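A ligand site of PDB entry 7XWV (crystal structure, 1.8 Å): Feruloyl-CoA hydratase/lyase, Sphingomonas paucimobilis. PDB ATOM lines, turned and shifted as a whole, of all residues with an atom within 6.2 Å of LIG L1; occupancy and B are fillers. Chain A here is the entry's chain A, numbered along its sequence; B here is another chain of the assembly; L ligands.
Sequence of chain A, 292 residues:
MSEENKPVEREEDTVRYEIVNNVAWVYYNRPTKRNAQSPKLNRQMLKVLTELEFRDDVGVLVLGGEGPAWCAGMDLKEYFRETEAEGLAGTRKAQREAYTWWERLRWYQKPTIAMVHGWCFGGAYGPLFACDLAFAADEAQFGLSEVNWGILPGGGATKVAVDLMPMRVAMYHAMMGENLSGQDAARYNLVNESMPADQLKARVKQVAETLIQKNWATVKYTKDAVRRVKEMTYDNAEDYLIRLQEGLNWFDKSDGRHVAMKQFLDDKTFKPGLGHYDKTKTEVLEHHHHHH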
ATOM      1  N   MET A  74      20.842   9.440  -1.321  1.00  0.00           N
ATOM      2  CA  MET A  74      21.731   8.661  -0.416  1.00  0.00           C
ATOM      3  C   MET A  74      21.181   8.690   1.022  1.00  0.00           C
ATOM      4  O   MET A  74      20.525   9.682   1.421  1.00  0.00           O
ATOM      5  CB  MET A  74      23.167   9.191  -0.428  1.00  0.00           C
ATOM      6  CG  MET A  74      23.717   9.500  -1.797  1.00  0.00           C
ATOM      7  SD  MET A  74      23.425   8.263  -3.050  1.00  0.00           S
ATOM      8  CE  MET A  74      24.411   6.837  -2.570  1.00  0.00           C
ATOM      9  N   TYR A  79      25.006   6.072   4.626  1.00  0.00           N
ATOM     10  CA  TYR A  79      25.965   6.412   3.526  1.00  0.00           C
ATOM     11  C   TYR A  79      26.930   7.550   3.912  1.00  0.00           C
ATOM     12  O   TYR A  79      28.123   7.458   3.509  1.00  0.00           O
ATOM     13  CB  TYR A  79      25.260   6.792   2.226  1.00  0.00           C
ATOM     14  CG  TYR A  79      26.200   7.033   1.080  1.00  0.00           C
ATOM     15  CD1 TYR A  79      26.771   6.002   0.349  1.00  0.00           C
ATOM     16  CD2 TYR A  79      26.474   8.332   0.671  1.00  0.00           C
ATOM     17  CE1 TYR A  79      27.624   6.256  -0.719  1.00  0.00           C
ATOM     18  CE2 TYR A  79      27.319   8.597  -0.392  1.00  0.00           C
ATOM     19  CZ  TYR A  79      27.880   7.568  -1.101  1.00  0.00           C
ATOM     20  OH  TYR A  79      28.696   7.897  -2.169  1.00  0.00           O
ATOM     21  N   PHE A  80      26.468   8.627   4.549  1.00  0.00           N
ATOM     22  CA  PHE A  80      27.309   9.826   4.834  1.00  0.00           C
ATOM     23  C   PHE A  80      27.892   9.766   6.264  1.00  0.00           C
ATOM     24  O   PHE A  80      29.118   9.564   6.386  1.00  0.00           O
ATOM     25  CB  PHE A  80      26.525  11.099   4.572  1.00  0.00           C
ATOM     26  CG  PHE A  80      26.305  11.429   3.111  1.00  0.00           C
ATOM     27  CD1 PHE A  80      27.378  11.636   2.244  1.00  0.00           C
ATOM     28  CD2 PHE A  80      25.027  11.625   2.619  1.00  0.00           C
ATOM     29  CE1 PHE A  80      27.160  11.961   0.914  1.00  0.00           C
ATOM     30  CE2 PHE A  80      24.803  11.969   1.298  1.00  0.00           C
ATOM     31  CZ  PHE A  80      25.866  12.119   0.436  1.00  0.00           C
ATOM     32  N   GLN A  95      31.579   5.447  -1.358  1.00  0.00           N
ATOM     33  CA  GLN A  95      31.517   6.075  -2.704  1.00  0.00           C
ATOM     34  C   GLN A  95      31.642   4.994  -3.815  1.00  0.00           C
ATOM     35  O   GLN A  95      30.856   4.989  -4.790  1.00  0.00           O
ATOM     36  CB  GLN A  95      32.615   7.124  -2.870  1.00  0.00           C
ATOM     37  CG  GLN A  95      32.343   8.390  -2.068  1.00  0.00           C
ATOM     38  CD  GLN A  95      33.502   9.353  -2.007  1.00  0.00           C
ATOM     39  OE1 GLN A  95      34.672   8.973  -2.102  1.00  0.00           O
ATOM     40  NE2 GLN A  95      33.175  10.605  -1.722  1.00  0.00           N
ATOM     41  N   ALA A  98      28.596   2.895  -4.558  1.00  0.00           N
ATOM     42  CA  ALA A  98      27.499   3.664  -5.194  1.00  0.00           C
ATOM     43  C   ALA A  98      27.855   3.813  -6.693  1.00  0.00           C
ATOM     44  O   ALA A  98      27.148   3.211  -7.532  1.00  0.00           O
ATOM     45  CB  ALA A  98      27.286   4.993  -4.502  1.00  0.00           C
ATOM     46  N   TYR A  99      29.015   4.425  -6.981  1.00  0.00           N
ATOM     47  CA  TYR A  99      29.466   4.747  -8.362  1.00  0.00           C
ATOM     48  C   TYR A  99      29.510   3.457  -9.188  1.00  0.00           C
ATOM     49  O   TYR A  99      29.211   3.536 -10.394  1.00  0.00           O
ATOM     50  CB  TYR A  99      30.811   5.502  -8.363  1.00  0.00           C
ATOM     51  CG  TYR A  99      30.692   6.935  -7.927  1.00  0.00           C
ATOM     52  CD1 TYR A  99      30.143   7.900  -8.770  1.00  0.00           C
ATOM     53  CD2 TYR A  99      31.162   7.354  -6.701  1.00  0.00           C
ATOM     54  CE1 TYR A  99      30.044   9.224  -8.373  1.00  0.00           C
ATOM     55  CE2 TYR A  99      31.042   8.669  -6.276  1.00  0.00           C
ATOM     56  CZ  TYR A  99      30.499   9.610  -7.119  1.00  0.00           C
ATOM     57  OH  TYR A  99      30.414  10.896  -6.694  1.00  0.00           O
ATOM     58  N   TRP A 102      25.940   2.286 -10.327  1.00  0.00           N
ATOM     59  CA  TRP A 102      25.409   3.257 -11.310  1.00  0.00           C
ATOM     60  C   TRP A 102      26.086   3.017 -12.662  1.00  0.00           C
ATOM     61  O   TRP A 102      25.395   3.036 -13.632  1.00  0.00           O
ATOM     62  CB  TRP A 102      25.549   4.717 -10.869  1.00  0.00           C
ATOM     63  CG  TRP A 102      24.981   5.051  -9.522  1.00  0.00           C
ATOM     64  CD1 TRP A 102      24.040   4.357  -8.818  1.00  0.00           C
ATOM     65  CD2 TRP A 102      25.408   6.130  -8.677  1.00  0.00           C
ATOM     66  NE1 TRP A 102      23.776   4.996  -7.643  1.00  0.00           N
ATOM     67  CE2 TRP A 102      24.587   6.104  -7.535  1.00  0.00           C
ATOM     68  CE3 TRP A 102      26.313   7.173  -8.825  1.00  0.00           C
ATOM     69  CZ2 TRP A 102      24.735   7.016  -6.486  1.00  0.00           C
ATOM     70  CZ3 TRP A 102      26.460   8.085  -7.798  1.00  0.00           C
ATOM     71  CH2 TRP A 102      25.682   8.010  -6.643  1.00  0.00           C
ATOM     72  N   GLY A 122      18.391  13.909  -5.543  1.00  0.00           N
ATOM     73  CA  GLY A 122      19.818  13.945  -5.199  1.00  0.00           C
ATOM     74  C   GLY A 122      20.568  12.830  -5.870  1.00  0.00           C
ATOM     75  O   GLY A 122      20.578  12.770  -7.122  1.00  0.00           O
ATOM     76  N   GLY A 123      21.222  12.008  -5.065  1.00  0.00           N
ATOM     77  CA  GLY A 123      21.903  10.761  -5.503  1.00  0.00           C
ATOM     78  C   GLY A 123      21.075   9.826  -6.371  1.00  0.00           C
ATOM     79  O   GLY A 123      21.635   8.950  -6.975  1.00  0.00           O
ATOM     80  N   GLU A 146      20.397  19.045  -2.615  1.00  0.00           N
ATOM     81  CA  GLU A 146      21.724  19.107  -1.978  1.00  0.00           C
ATOM     82  C   GLU A 146      21.973  20.548  -1.517  1.00  0.00           C
ATOM     83  O   GLU A 146      22.429  20.727  -0.348  1.00  0.00           O
ATOM     84  CB  GLU A 146      22.790  18.667  -2.970  1.00  0.00           C
ATOM     85  CG  GLU A 146      22.772  17.181  -3.239  1.00  0.00           C
ATOM     86  CD  GLU A 146      22.064  16.686  -4.493  1.00  0.00           C
ATOM     87  OE1 GLU A 146      22.477  15.603  -5.003  1.00  0.00           O
ATOM     88  OE2 GLU A 146      21.063  17.344  -4.931  1.00  0.00           O
ATOM     89  N   TRP A 149      20.740  21.275   1.826  1.00  0.00           N
ATOM     90  CA  TRP A 149      21.462  20.830   3.042  1.00  0.00           C
ATOM     91  C   TRP A 149      22.966  21.131   2.917  1.00  0.00           C
ATOM     92  O   TRP A 149      23.765  20.500   3.642  1.00  0.00           O
ATOM     93  CB  TRP A 149      21.061  19.390   3.422  1.00  0.00           C
ATOM     94  CG  TRP A 149      21.331  18.243   2.487  1.00  0.00           C
ATOM     95  CD1 TRP A 149      20.578  17.812   1.426  1.00  0.00           C
ATOM     96  CD2 TRP A 149      22.368  17.254   2.664  1.00  0.00           C
ATOM     97  NE1 TRP A 149      21.114  16.674   0.887  1.00  0.00           N
ATOM     98  CE2 TRP A 149      22.213  16.303   1.629  1.00  0.00           C
ATOM     99  CE3 TRP A 149      23.418  17.092   3.578  1.00  0.00           C
ATOM    100  CZ2 TRP A 149      23.085  15.230   1.482  1.00  0.00           C
ATOM    101  CZ3 TRP A 149      24.291  16.028   3.434  1.00  0.00           C
ATOM    102  CH2 TRP A 149      24.113  15.118   2.395  1.00  0.00           C
ATOM    103  N   ILE A 151      25.414  21.105   0.521  1.00  0.00           N
ATOM    104  CA  ILE A 151      26.407  20.408  -0.350  1.00  0.00           C
ATOM    105  C   ILE A 151      26.070  20.600  -1.826  1.00  0.00           C
ATOM    106  O   ILE A 151      24.907  20.957  -2.159  1.00  0.00           O
ATOM    107  CB  ILE A 151      26.554  18.919  -0.016  1.00  0.00           C
ATOM    108  CG1 ILE A 151      25.370  18.114  -0.591  1.00  0.00           C
ATOM    109  CG2 ILE A 151      26.761  18.737   1.491  1.00  0.00           C
ATOM    110  CD1 ILE A 151      25.438  16.641  -0.331  1.00  0.00           C
ATOM    111  N   LEU A 152      27.125  20.471  -2.640  1.00  0.00           N
ATOM    112  CA  LEU A 152      27.145  20.385  -4.125  1.00  0.00           C
ATOM    113  C   LEU A 152      26.310  19.186  -4.553  1.00  0.00           C
ATOM    114  O   LEU A 152      26.452  18.137  -3.938  1.00  0.00           O
ATOM    115  CB  LEU A 152      28.590  20.123  -4.602  1.00  0.00           C
ATOM    116  CG  LEU A 152      29.462  21.341  -4.892  1.00  0.00           C
ATOM    117  CD1 LEU A 152      30.880  21.083  -4.420  1.00  0.00           C
ATOM    118  CD2 LEU A 152      29.456  21.673  -6.372  1.00  0.00           C
ATOM    119  N   PRO A 153      25.563  19.251  -5.670  1.00  0.00           N
ATOM    120  CA  PRO A 153      24.927  18.045  -6.233  1.00  0.00           C
ATOM    121  C   PRO A 153      25.996  17.041  -6.723  1.00  0.00           C
ATOM    122  O   PRO A 153      26.477  17.155  -7.845  1.00  0.00           O
ATOM    123  CB  PRO A 153      24.058  18.568  -7.388  1.00  0.00           C
ATOM    124  CG  PRO A 153      23.939  20.082  -7.147  1.00  0.00           C
ATOM    125  CD  PRO A 153      25.242  20.459  -6.476  1.00  0.00           C
ATOM    126  N   GLY A 154      26.333  16.087  -5.865  1.00  0.00           N
ATOM    127  CA  GLY A 154      27.411  15.101  -6.115  1.00  0.00           C
ATOM    128  C   GLY A 154      26.881  13.811  -6.733  1.00  0.00           C
ATOM    129  O   GLY A 154      25.695  13.778  -7.182  1.00  0.00           O
ATOM    130  N   GLY A 155      27.667  12.745  -6.672  1.00  0.00           N
ATOM    131  CA  GLY A 155      27.321  11.466  -7.318  1.00  0.00           C
ATOM    132  C   GLY A 155      27.000  11.687  -8.791  1.00  0.00           C
ATOM    133  O   GLY A 155      26.166  10.958  -9.310  1.00  0.00           O
ATOM    134  N   GLY A 156      27.643  12.696  -9.400  1.00  0.00           N
ATOM    135  CA  GLY A 156      27.459  13.049 -10.804  1.00  0.00           C
ATOM    136  C   GLY A 156      26.178  13.819 -11.085  1.00  0.00           C
ATOM    137  O   GLY A 156      25.962  14.130 -12.245  1.00  0.00           O
ATOM    138  N   ALA A 157      25.373  14.127 -10.085  1.00  0.00           N
ATOM    139  CA  ALA A 157      24.020  14.658 -10.305  1.00  0.00           C
ATOM    140  C   ALA A 157      24.100  16.000 -11.059  1.00  0.00           C
ATOM    141  O   ALA A 157      23.157  16.338 -11.796  1.00  0.00           O
ATOM    142  CB  ALA A 157      23.271  14.787  -8.998  1.00  0.00           C
ATOM    143  N   GLN B 245      33.737  19.246  -3.779  1.00  0.00           N
ATOM    144  CA  GLN B 245      33.109  19.127  -2.425  1.00  0.00           C
ATOM    145  C   GLN B 245      34.183  19.248  -1.334  1.00  0.00           C
ATOM    146  O   GLN B 245      33.863  19.820  -0.305  1.00  0.00           O
ATOM    147  CB  GLN B 245      32.211  17.901  -2.295  1.00  0.00           C
ATOM    148  CG  GLN B 245      31.585  17.737  -0.918  1.00  0.00           C
ATOM    149  CD  GLN B 245      30.611  18.846  -0.638  1.00  0.00           C
ATOM    150  OE1 GLN B 245      29.629  19.019  -1.367  1.00  0.00           O
ATOM    151  NE2 GLN B 245      30.890  19.638   0.396  1.00  0.00           N
HETATM  152  C1  LIG L   1      25.734  12.615  -3.657  1.00  0.00           C
HETATM  153  C2  LIG L   1      26.798  13.181  -2.935  1.00  0.00           C
HETATM  154  C3  LIG L   1      27.914  12.442  -2.605  1.00  0.00           C
HETATM  155  C4  LIG L   1      27.945  11.073  -2.928  1.00  0.00           C
HETATM  156  C5  LIG L   1      26.903  10.508  -3.615  1.00  0.00           C
HETATM  157  O1  LIG L   1      24.441  14.580  -4.037  1.00  0.00           O
HETATM  158  C6  LIG L   1      25.803  11.280  -3.973  1.00  0.00           C
HETATM  159  C7  LIG L   1      24.550  13.370  -4.039  1.00  0.00           C
HETATM  160  C8  LIG L   1      29.041  14.209  -1.433  1.00  0.00           C
HETATM  161  O2  LIG L   1      29.044  12.877  -1.939  1.00  0.00           O
HETATM  162  O3  LIG L   1      29.015  10.305  -2.591  1.00  0.00           O
HETATM  163  N1  LG2 L   2      18.272   9.429   3.853  1.00  0.00           N
HETATM  164  C1  LG2 L   2      17.945   8.759   4.969  1.00  0.00           C
HETATM  165  N2  LG2 L   2      16.747   8.579   5.522  1.00  0.00           N
HETATM  166  C2  LG2 L   2      15.800   9.174   4.792  1.00  0.00           C
HETATM  167  C3  LG2 L   2      15.962   9.898   3.625  1.00  0.00           C
HETATM  168  C4  LG2 L   2      17.285  10.031   3.146  1.00  0.00           C
HETATM  169  N3  LG2 L   2      17.611  10.691   2.026  1.00  0.00           N
HETATM  170  N4  LG2 L   2      14.736  10.372   3.166  1.00  0.00           N
HETATM  171  C5  LG2 L   2      13.864   9.930   4.046  1.00  0.00           C
HETATM  172  N5  LG2 L   2      14.460   9.202   5.057  1.00  0.00           N
HETATM  173  C6  LG2 L   2      13.833   8.555   6.200  1.00  0.00           C
HETATM  174  C7  LG2 L   2      13.304   9.484   7.294  1.00  0.00           C
HETATM  175  O1  LG2 L   2      14.285   9.781   8.262  1.00  0.00           O
HETATM  176  C8  LG2 L   2      12.189   8.626   7.869  1.00  0.00           C
HETATM  177  O2  LG2 L   2      12.789   7.615   8.694  1.00  0.00           O
HETATM  178  P1  LG2 L   2      12.106   7.350  10.142  1.00  0.00           P
HETATM  179  O3  LG2 L   2      12.873   8.333  11.029  1.00  0.00           O
HETATM  180  O4  LG2 L   2      10.616   7.660  10.087  1.00  0.00           O
HETATM  181  O5  LG2 L   2      12.384   5.902  10.503  1.00  0.00           O
HETATM  182  C9  LG2 L   2      11.585   7.977   6.616  1.00  0.00           C
HETATM  183  O6  LG2 L   2      12.710   7.855   5.710  1.00  0.00           O
HETATM  184  C10 LG2 L   2      10.483   8.726   5.905  1.00  0.00           C
HETATM  185  O7  LG2 L   2      10.070   9.831   6.724  1.00  0.00           O
HETATM  186  P2  LG2 L   2       9.604  11.229   6.096  1.00  0.00           P
HETATM  187  O8  LG2 L   2      10.793  12.067   5.793  1.00  0.00           O
HETATM  188  O9  LG2 L   2       8.559  11.799   6.994  1.00  0.00           O
HETATM  189  O10 LG2 L   2       8.902  10.788   4.703  1.00  0.00           O
HETATM  190  P3  LG2 L   2       7.882  11.579   3.729  1.00  0.00           P
HETATM  191  O11 LG2 L   2       7.094  12.578   4.521  1.00  0.00           O
HETATM  192  O12 LG2 L   2       7.159  10.606   2.850  1.00  0.00           O
HETATM  193  O13 LG2 L   2       8.878  12.439   2.818  1.00  0.00           O
HETATM  194  C11 LG2 L   2      10.781  12.650   1.350  1.00  0.00           C
HETATM  195  C12 LG2 L   2       9.627  11.763   1.787  1.00  0.00           C
HETATM  196  C13 LG2 L   2      11.619  11.845   0.342  1.00  0.00           C
HETATM  197  C14 LG2 L   2      10.196  13.903   0.671  1.00  0.00           C
HETATM  198  C15 LG2 L   2      11.670  13.087   2.532  1.00  0.00           C
HETATM  199  O14 LG2 L   2      11.956  11.964   3.342  1.00  0.00           O
HETATM  200  C16 LG2 L   2      12.964  13.786   2.126  1.00  0.00           C
HETATM  201  O15 LG2 L   2      12.975  15.006   1.941  1.00  0.00           O
HETATM  202  N6  LG2 L   2      14.057  13.038   2.010  1.00  0.00           N
HETATM  203  C17 LG2 L   2      15.399  13.579   1.821  1.00  0.00           C
HETATM  204  C18 LG2 L   2      15.771  13.750   0.365  1.00  0.00           C
HETATM  205  C19 LG2 L   2      17.201  14.260   0.255  1.00  0.00           C
HETATM  206  O16 LG2 L   2      17.537  15.258   0.881  1.00  0.00           O
HETATM  207  N7  LG2 L   2      18.074  13.561  -0.492  1.00  0.00           N
HETATM  208  C20 LG2 L   2      19.515  13.835  -0.512  1.00  0.00           C
HETATM  209  C21 LG2 L   2      20.378  12.593  -0.584  1.00  0.00           C
HETATM  210  S1  LG2 L   2      21.515  12.550  -1.993  1.00  0.00           S
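O of Glu 146 sits at hydrogen-bond distance from N of Ile 151 (3.1 Å).
The side-chain hydroxyl (OH) of Tyr 99 sits close to the backbone NH (N) of Gly 155, at 3.3 Å.
An oxygen (O1) of LIG L1 sits close to the side-chain carboxylate (OE1) of Glu 146, at 2.4 Å.
OH of Tyr 79 sits at hydrogen-bond distance from O3 of LIG L1 (2.5 Å).
The backbone NH of Gly 154 is in hydrogen-bond range of an oxygen (O1) of LIG L1 (3.0 Å).
A sulfur (S1) of LG2 L2 lies close to the backbone NH (N) of Met 74 (3.3 Å).
A nitrogen (N3) of LG2 L2 sits at hydrogen-bond distance from the backbone carbonyl oxygen (O) of Met 74, at 3.1 Å.
The backbone NH (N) of Gly 123 lies close to a sulfur (S1) of LG2 L2.
Met 74 touches LIG L1 (CG to C6, 3.5 Å).
Phe 80 touches LIG L1.
Gln 95 touches LIG L1.
Gly 123 touches LIG L1.
Pro 153 touches LIG L1.
Gly 155 touches LIG L1 (N to C1, 3.6 Å).
Hydrophobic or aromatic side chains within 4 Å of LIG L1: Met 74, Tyr 79 and Phe 80.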
